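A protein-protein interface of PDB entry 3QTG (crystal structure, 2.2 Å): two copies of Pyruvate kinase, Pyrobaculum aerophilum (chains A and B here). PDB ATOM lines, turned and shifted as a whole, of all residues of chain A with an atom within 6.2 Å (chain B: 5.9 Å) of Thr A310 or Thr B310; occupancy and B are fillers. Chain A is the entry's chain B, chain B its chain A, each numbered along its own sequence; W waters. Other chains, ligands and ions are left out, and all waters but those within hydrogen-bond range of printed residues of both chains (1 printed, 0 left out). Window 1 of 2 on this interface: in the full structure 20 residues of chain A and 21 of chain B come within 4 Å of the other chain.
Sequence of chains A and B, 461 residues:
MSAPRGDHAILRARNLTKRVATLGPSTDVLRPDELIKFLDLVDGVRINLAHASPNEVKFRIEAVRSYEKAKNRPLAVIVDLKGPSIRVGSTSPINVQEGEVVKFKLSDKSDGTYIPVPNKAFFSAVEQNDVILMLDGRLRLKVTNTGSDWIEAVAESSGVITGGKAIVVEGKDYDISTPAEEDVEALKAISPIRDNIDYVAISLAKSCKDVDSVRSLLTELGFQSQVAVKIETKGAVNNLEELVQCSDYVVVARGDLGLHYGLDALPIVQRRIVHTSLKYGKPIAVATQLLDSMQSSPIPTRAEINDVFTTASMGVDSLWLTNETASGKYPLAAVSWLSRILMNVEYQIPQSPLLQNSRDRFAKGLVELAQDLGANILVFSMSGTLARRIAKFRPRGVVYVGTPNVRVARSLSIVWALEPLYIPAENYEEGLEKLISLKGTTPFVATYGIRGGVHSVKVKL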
ATOM      1  N   GLN A 270      15.210  18.641  37.811  1.00  0.00           N
ATOM      2  CA  GLN A 270      15.594  17.474  37.022  1.00  0.00           C
ATOM      3  C   GLN A 270      16.219  17.924  35.706  1.00  0.00           C
ATOM      4  O   GLN A 270      17.243  17.402  35.274  1.00  0.00           O
ATOM      5  CB  GLN A 270      14.389  16.565  36.761  1.00  0.00           C
ATOM      6  CG  GLN A 270      14.682  15.393  35.803  1.00  0.00           C
ATOM      7  CD  GLN A 270      13.468  14.479  35.592  1.00  0.00           C
ATOM      8  OE1 GLN A 270      12.833  14.033  36.552  1.00  0.00           O
ATOM      9  NE2 GLN A 270      13.157  14.191  34.342  1.00  0.00           N
ATOM     10  N   ARG A 271      15.591  18.905  35.075  1.00  0.00           N
ATOM     11  CA  ARG A 271      16.073  19.405  33.792  1.00  0.00           C
ATOM     12  C   ARG A 271      17.458  20.051  33.880  1.00  0.00           C
ATOM     13  O   ARG A 271      18.307  19.815  33.024  1.00  0.00           O
ATOM     14  CB  ARG A 271      15.050  20.360  33.181  1.00  0.00           C
ATOM     15  CG  ARG A 271      15.218  20.545  31.711  1.00  0.00           C
ATOM     16  CD  ARG A 271      14.504  21.800  31.204  1.00  0.00           C
ATOM     17  NE  ARG A 271      13.084  21.573  30.983  1.00  0.00           N
ATOM     18  CZ  ARG A 271      12.358  22.232  30.081  1.00  0.00           C
ATOM     19  NH1 ARG A 271      11.066  21.958  29.932  1.00  0.00           N
ATOM     20  NH2 ARG A 271      12.926  23.162  29.318  1.00  0.00           N
ATOM     21  N   ILE A 305       3.377   6.888  31.990  1.00  0.00           N
ATOM     22  CA  ILE A 305       3.857   6.620  30.640  1.00  0.00           C
ATOM     23  C   ILE A 305       4.427   7.899  30.012  1.00  0.00           C
ATOM     24  O   ILE A 305       5.506   7.873  29.445  1.00  0.00           O
ATOM     25  CB  ILE A 305       2.709   6.014  29.743  1.00  0.00           C
ATOM     26  CG1 ILE A 305       2.490   4.533  30.065  1.00  0.00           C
ATOM     27  CG2 ILE A 305       3.002   6.186  28.255  1.00  0.00           C
ATOM     28  CD1 ILE A 305       1.092   4.055  29.690  1.00  0.00           C
ATOM     29  N   ASN A 306       3.701   9.005  30.119  1.00  0.00           N
ATOM     30  CA  ASN A 306       4.157  10.301  29.589  1.00  0.00           C
ATOM     31  C   ASN A 306       5.446  10.773  30.263  1.00  0.00           C
ATOM     32  O   ASN A 306       6.377  11.189  29.597  1.00  0.00           O
ATOM     33  CB  ASN A 306       3.063  11.378  29.712  1.00  0.00           C
ATOM     34  CG  ASN A 306       1.894  11.155  28.740  1.00  0.00           C
ATOM     35  OD1 ASN A 306       0.701  11.155  29.134  1.00  0.00           O
ATOM     36  ND2 ASN A 306       2.222  10.988  27.466  1.00  0.00           N
ATOM     37  N   ASP A 307       5.484  10.674  31.584  1.00  0.00           N
ATOM     38  CA  ASP A 307       6.663  11.007  32.409  1.00  0.00           C
ATOM     39  C   ASP A 307       7.875  10.169  32.000  1.00  0.00           C
ATOM     40  O   ASP A 307       8.962  10.712  31.790  1.00  0.00           O
ATOM     41  CB  ASP A 307       6.299  10.791  33.884  1.00  0.00           C
ATOM     42  CG  ASP A 307       7.375  11.253  34.861  1.00  0.00           C
ATOM     43  OD1 ASP A 307       8.327  11.991  34.480  1.00  0.00           O
ATOM     44  OD2 ASP A 307       7.243  10.850  36.049  1.00  0.00           O
ATOM     45  N   VAL A 308       7.696   8.856  31.852  1.00  0.00           N
ATOM     46  CA  VAL A 308       8.806   8.005  31.418  1.00  0.00           C
ATOM     47  C   VAL A 308       9.262   8.418  30.029  1.00  0.00           C
ATOM     48  O   VAL A 308      10.463   8.482  29.780  1.00  0.00           O
ATOM     49  CB  VAL A 308       8.459   6.495  31.407  1.00  0.00           C
ATOM     50  CG1 VAL A 308       9.539   5.672  30.641  1.00  0.00           C
ATOM     51  CG2 VAL A 308       8.301   5.985  32.807  1.00  0.00           C
ATOM     52  N   PHE A 309       8.294   8.672  29.136  1.00  0.00           N
ATOM     53  CA  PHE A 309       8.568   8.988  27.753  1.00  0.00           C
ATOM     54  C   PHE A 309       9.353  10.297  27.602  1.00  0.00           C
ATOM     55  O   PHE A 309      10.330  10.341  26.858  1.00  0.00           O
ATOM     56  CB  PHE A 309       7.256   9.078  26.950  1.00  0.00           C
ATOM     57  CG  PHE A 309       7.451   9.466  25.507  1.00  0.00           C
ATOM     58  CD1 PHE A 309       7.472   8.496  24.509  1.00  0.00           C
ATOM     59  CD2 PHE A 309       7.612  10.799  25.144  1.00  0.00           C
ATOM     60  CE1 PHE A 309       7.640   8.850  23.182  1.00  0.00           C
ATOM     61  CE2 PHE A 309       7.795  11.150  23.796  1.00  0.00           C
ATOM     62  CZ  PHE A 309       7.809  10.172  22.830  1.00  0.00           C
ATOM     63  N   THR A 310       8.910  11.351  28.299  1.00  0.00           N
ATOM     64  CA  THR A 310       9.519  12.683  28.193  1.00  0.00           C
ATOM     65  C   THR A 310      10.890  12.708  28.880  1.00  0.00           C
ATOM     66  O   THR A 310      11.816  13.386  28.428  1.00  0.00           O
ATOM     67  CB  THR A 310       8.590  13.789  28.755  1.00  0.00           C
ATOM     68  OG1 THR A 310       8.359  13.544  30.139  1.00  0.00           O
ATOM     69  CG2 THR A 310       7.209  13.808  28.030  1.00  0.00           C
ATOM     70  N   THR A 311      11.028  11.939  29.952  1.00  0.00           N
ATOM     71  CA  THR A 311      12.311  11.835  30.639  1.00  0.00           C
ATOM     72  C   THR A 311      13.330  11.120  29.752  1.00  0.00           C
ATOM     73  O   THR A 311      14.442  11.614  29.598  1.00  0.00           O
ATOM     74  CB  THR A 311      12.180  11.127  32.010  1.00  0.00           C
ATOM     75  OG1 THR A 311      11.477  11.989  32.909  1.00  0.00           O
ATOM     76  CG2 THR A 311      13.557  10.780  32.593  1.00  0.00           C
ATOM     77  N   ALA A 312      12.957   9.979  29.160  1.00  0.00           N
ATOM     78  CA  ALA A 312      13.840   9.307  28.193  1.00  0.00           C
ATOM     79  C   ALA A 312      14.187  10.212  26.999  1.00  0.00           C
ATOM     80  O   ALA A 312      15.318  10.258  26.561  1.00  0.00           O
ATOM     81  CB  ALA A 312      13.219   8.007  27.697  1.00  0.00           C
ATOM     82  N   SER A 313      13.181  10.906  26.476  1.00  0.00           N
ATOM     83  CA  SER A 313      13.338  11.787  25.327  1.00  0.00           C
ATOM     84  C   SER A 313      14.420  12.876  25.512  1.00  0.00           C
ATOM     85  O   SER A 313      15.023  13.288  24.531  1.00  0.00           O
ATOM     86  CB  SER A 313      11.980  12.406  24.971  1.00  0.00           C
ATOM     87  OG  SER A 313      12.079  13.251  23.847  1.00  0.00           O
ATOM     88  N   MET A 314      14.638  13.337  26.752  1.00  0.00           N
ATOM     89  CA  MET A 314      15.733  14.286  27.096  1.00  0.00           C
ATOM     90  C   MET A 314      17.163  13.774  26.795  1.00  0.00           C
ATOM     91  O   MET A 314      18.115  14.572  26.693  1.00  0.00           O
ATOM     92  CB  MET A 314      15.713  14.614  28.590  1.00  0.00           C
ATOM     93  CG  MET A 314      14.514  15.365  29.115  1.00  0.00           C
ATOM     94  SD  MET A 314      14.795  15.549  30.911  1.00  0.00           S
ATOM     95  CE  MET A 314      15.685  17.086  30.887  1.00  0.00           C
ATOM     96  N   GLY A 315      17.329  12.458  26.707  1.00  0.00           N
ATOM     97  CA  GLY A 315      18.614  11.871  26.323  1.00  0.00           C
ATOM     98  C   GLY A 315      19.421  11.290  27.478  1.00  0.00           C
ATOM     99  O   GLY A 315      20.622  11.150  27.373  1.00  0.00           O
ATOM    100  N   VAL A 345      10.040   5.827  22.073  1.00  0.00           N
ATOM    101  CA  VAL A 345      10.649   7.141  22.294  1.00  0.00           C
ATOM    102  C   VAL A 345      11.278   7.712  21.021  1.00  0.00           C
ATOM    103  O   VAL A 345      12.014   7.024  20.312  1.00  0.00           O
ATOM    104  CB  VAL A 345      11.702   7.111  23.454  1.00  0.00           C
ATOM    105  CG1 VAL A 345      12.505   8.428  23.519  1.00  0.00           C
ATOM    106  CG2 VAL A 345      11.018   6.832  24.778  1.00  0.00           C
ATOM    107  N   ARG B 271       2.726  14.567  20.168  1.00  0.00           N
ATOM    108  CA  ARG B 271       3.826  15.373  19.660  1.00  0.00           C
ATOM    109  C   ARG B 271       3.605  15.723  18.193  1.00  0.00           C
ATOM    110  O   ARG B 271       3.772  16.871  17.804  1.00  0.00           O
ATOM    111  CB  ARG B 271       5.159  14.643  19.870  1.00  0.00           C
ATOM    112  CG  ARG B 271       6.356  15.455  19.549  1.00  0.00           C
ATOM    113  CD  ARG B 271       7.614  14.586  19.552  1.00  0.00           C
ATOM    114  NE  ARG B 271       8.087  14.306  20.900  1.00  0.00           N
ATOM    115  CZ  ARG B 271       9.251  13.720  21.169  1.00  0.00           C
ATOM    116  NH1 ARG B 271      10.055  13.348  20.181  1.00  0.00           N
ATOM    117  NH2 ARG B 271       9.616  13.513  22.428  1.00  0.00           N
ATOM    118  N   ILE B 305       1.971  16.111  37.475  1.00  0.00           N
ATOM    119  CA  ILE B 305       2.746  17.355  37.449  1.00  0.00           C
ATOM    120  C   ILE B 305       3.791  17.331  36.316  1.00  0.00           C
ATOM    121  O   ILE B 305       3.849  18.254  35.526  1.00  0.00           O
ATOM    122  CB  ILE B 305       3.411  17.654  38.830  1.00  0.00           C
ATOM    123  CG1 ILE B 305       2.329  17.998  39.871  1.00  0.00           C
ATOM    124  CG2 ILE B 305       4.457  18.763  38.710  1.00  0.00           C
ATOM    125  CD1 ILE B 305       2.706  17.694  41.297  1.00  0.00           C
ATOM    126  N   ASN B 306       4.604  16.283  36.229  1.00  0.00           N
ATOM    127  CA  ASN B 306       5.536  16.174  35.098  1.00  0.00           C
ATOM    128  C   ASN B 306       4.839  16.218  33.712  1.00  0.00           C
ATOM    129  O   ASN B 306       5.319  16.903  32.804  1.00  0.00           O
ATOM    130  CB  ASN B 306       6.428  14.944  35.227  1.00  0.00           C
ATOM    131  CG  ASN B 306       7.433  15.065  36.361  1.00  0.00           C
ATOM    132  OD1 ASN B 306       7.499  14.207  37.253  1.00  0.00           O
ATOM    133  ND2 ASN B 306       8.231  16.117  36.331  1.00  0.00           N
ATOM    134  N   ASP B 307       3.715  15.507  33.580  1.00  0.00           N
ATOM    135  CA  ASP B 307       2.889  15.487  32.342  1.00  0.00           C
ATOM    136  C   ASP B 307       2.444  16.895  31.900  1.00  0.00           C
ATOM    137  O   ASP B 307       2.702  17.305  30.767  1.00  0.00           O
ATOM    138  CB  ASP B 307       1.682  14.568  32.554  1.00  0.00           C
ATOM    139  CG  ASP B 307       0.930  14.233  31.260  1.00  0.00           C
ATOM    140  OD1 ASP B 307       1.415  14.546  30.148  1.00  0.00           O
ATOM    141  OD2 ASP B 307      -0.173  13.638  31.374  1.00  0.00           O
ATOM    142  N   VAL B 308       1.821  17.641  32.810  1.00  0.00           N
ATOM    143  CA  VAL B 308       1.407  19.022  32.549  1.00  0.00           C
ATOM    144  C   VAL B 308       2.626  19.901  32.235  1.00  0.00           C
ATOM    145  O   VAL B 308       2.588  20.725  31.312  1.00  0.00           O
ATOM    146  CB  VAL B 308       0.639  19.632  33.758  1.00  0.00           C
ATOM    147  CG1 VAL B 308       0.298  21.142  33.526  1.00  0.00           C
ATOM    148  CG2 VAL B 308      -0.624  18.846  34.047  1.00  0.00           C
ATOM    149  N   PHE B 309       3.693  19.734  33.027  1.00  0.00           N
ATOM    150  CA  PHE B 309       4.881  20.542  32.853  1.00  0.00           C
ATOM    151  C   PHE B 309       5.419  20.328  31.425  1.00  0.00           C
ATOM    152  O   PHE B 309       5.630  21.278  30.713  1.00  0.00           O
ATOM    153  CB  PHE B 309       5.936  20.228  33.920  1.00  0.00           C
ATOM    154  CG  PHE B 309       7.199  21.037  33.778  1.00  0.00           C
ATOM    155  CD1 PHE B 309       7.347  22.245  34.461  1.00  0.00           C
ATOM    156  CD2 PHE B 309       8.227  20.606  32.943  1.00  0.00           C
ATOM    157  CE1 PHE B 309       8.513  22.996  34.327  1.00  0.00           C
ATOM    158  CE2 PHE B 309       9.397  21.358  32.787  1.00  0.00           C
ATOM    159  CZ  PHE B 309       9.538  22.549  33.479  1.00  0.00           C
ATOM    160  N   THR B 310       5.590  19.083  31.001  1.00  0.00           N
ATOM    161  CA  THR B 310       6.180  18.808  29.684  1.00  0.00           C
ATOM    162  C   THR B 310       5.254  19.095  28.485  1.00  0.00           C
ATOM    163  O   THR B 310       5.706  19.553  27.430  1.00  0.00           O
ATOM    164  CB  THR B 310       6.756  17.387  29.604  1.00  0.00           C
ATOM    165  OG1 THR B 310       5.743  16.447  29.953  1.00  0.00           O
ATOM    166  CG2 THR B 310       7.910  17.213  30.578  1.00  0.00           C
ATOM    167  N   THR B 311       3.965  18.836  28.637  1.00  0.00           N
ATOM    168  CA  THR B 311       2.988  19.242  27.616  1.00  0.00           C
ATOM    169  C   THR B 311       3.029  20.766  27.370  1.00  0.00           C
ATOM    170  O   THR B 311       3.122  21.204  26.212  1.00  0.00           O
ATOM    171  CB  THR B 311       1.570  18.742  27.996  1.00  0.00           C
ATOM    172  OG1 THR B 311       1.591  17.305  28.037  1.00  0.00           O
ATOM    173  CG2 THR B 311       0.522  19.194  27.003  1.00  0.00           C
ATOM    174  N   ALA B 312       2.983  21.557  28.452  1.00  0.00           N
ATOM    175  CA  ALA B 312       3.106  23.011  28.348  1.00  0.00           C
ATOM    176  C   ALA B 312       4.432  23.491  27.717  1.00  0.00           C
ATOM    177  O   ALA B 312       4.419  24.449  26.935  1.00  0.00           O
ATOM    178  CB  ALA B 312       2.866  23.699  29.706  1.00  0.00           C
ATOM    179  N   SER B 313       5.546  22.832  28.063  1.00  0.00           N
ATOM    180  CA  SER B 313       6.883  23.120  27.495  1.00  0.00           C
ATOM    181  C   SER B 313       6.975  23.035  25.990  1.00  0.00           C
ATOM    182  O   SER B 313       7.798  23.720  25.390  1.00  0.00           O
ATOM    183  CB  SER B 313       7.934  22.152  28.048  1.00  0.00           C
ATOM    184  OG  SER B 313       8.234  22.495  29.374  1.00  0.00           O
ATOM    185  N   MET B 314       6.164  22.159  25.393  1.00  0.00           N
ATOM    186  CA  MET B 314       6.121  21.993  23.938  1.00  0.00           C
ATOM    187  C   MET B 314       5.658  23.270  23.262  1.00  0.00           C
ATOM    188  O   MET B 314       5.847  23.444  22.065  1.00  0.00           O
ATOM    189  CB  MET B 314       5.141  20.893  23.542  1.00  0.00           C
ATOM    190  CG  MET B 314       5.560  19.470  23.817  1.00  0.00           C
ATOM    191  SD  MET B 314       4.350  18.370  23.007  1.00  0.00           S
ATOM    192  CE  MET B 314       5.071  18.338  21.367  1.00  0.00           C
ATOM    193  N   GLY B 315       5.017  24.146  24.029  1.00  0.00           N
ATOM    194  CA  GLY B 315       4.572  25.439  23.516  1.00  0.00           C
ATOM    195  C   GLY B 315       3.131  25.469  23.023  1.00  0.00           C
ATOM    196  O   GLY B 315       2.799  26.288  22.180  1.00  0.00           O
HETATM  197  O   HOH W   1      10.815  15.581  38.050  1.00  0.00           O
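The side-chain hydroxyl of Ser A313 lies within hydrogen-bond range of the guanidinium group of Arg B271 (2.9 Å).
The side-chain carboxylate of Asp B307 sits close to the side-chain amide oxygen of Asn A306 (3.5 Å).
The guanidinium group (NH1) of Arg A271 sits at hydrogen-bond distance from the side-chain hydroxyl (OG) of Ser B313, 2.9 Å away.
The backbone carbonyl oxygen (O) of Asn B306 lies within hydrogen-bond range of the side-chain hydroxyl (OG1) of Thr B310 (2.9 Å).
The backbone carbonyl oxygen (O) of Asp B307 sits at hydrogen-bond distance from the side-chain hydroxyl (OG1) of Thr B310.
OG of Ser B313 lies within hydrogen-bond range of O of Phe B309.
OG1 of Thr A310 sits at hydrogen-bond distance from O of Asn A306 (3.1 Å).
The backbone carbonyl oxygen (O) of Asp A307 sits at hydrogen-bond distance from the side-chain hydroxyl (OG1) of Thr A310.
The backbone carbonyl oxygen (O) of Asp A307 lies within hydrogen-bond range of the side-chain hydroxyl (OG1) of Thr A311 (3.0 Å).
NH1 of Arg A271 touches CE2 of Phe B309, at 3.4 Å.
OD2 of Asp A307 touches OD1 of Asn B306, at 3.6 Å.
Phe A309 touches Arg B271 (CE2 to NH2, 3.3 Å).
Thr A310 touches Thr B310.
Thr A310 touches just one residue of chain B: Thr B310.
Printed residues of chain A within 4 Å of Arg B271: Phe A309 and Ser A313.
Printed residues of chain A within 4 Å of Asn B306: Asp A307 (3.6 Å).
Ala B312 touches none of the printed residues of chain A.
The nearest residue of chain B that does not touch Thr A310 is Asn B306 (5.3 Å).
The nearest printed residue of chain A that does not touch Arg B271 is Thr A310 (5.8 Å).
Hydrophobic or aromatic side chains of chain A that line the printed part of chain B: Phe A309.
Of the 12 printed residues of chain B, 6 touch a printed residue of chain A.
Among the printed residues, 7 pairs touch across the chains.
Among the printed residues, no Asp or Glu carboxylate lies within 4 Å of a Lys or Arg side-chain nitrogen of the other chain.
Arg A271 touches Phe B309, and with the chains exchanged Phe A309 touches Arg B271.
Arg A271 touches Ser B313, and with the chains exchanged Ser A313 touches Arg B271.
Asn A306 touches Asp B307, and with the chains exchanged Asp A307 touches Asn B306.
Thr B310 touches its own counterpart, Thr A310.
Positions printed for both chains: 271, 305, 306, 307, 308, 309, 310, 311, 312, 313, 314 and 315.
Of the 7 pairs that touch across the chains among the printed residues, 7 have their exchanged pair printed and touching as well.
Water W1 lies within hydrogen-bond range of the side-chain amide oxygen (OE1) of Gln A270 (3.0 Å) and the side-chain amide nitrogen (ND2) of Asn B306 (3.1 Å).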
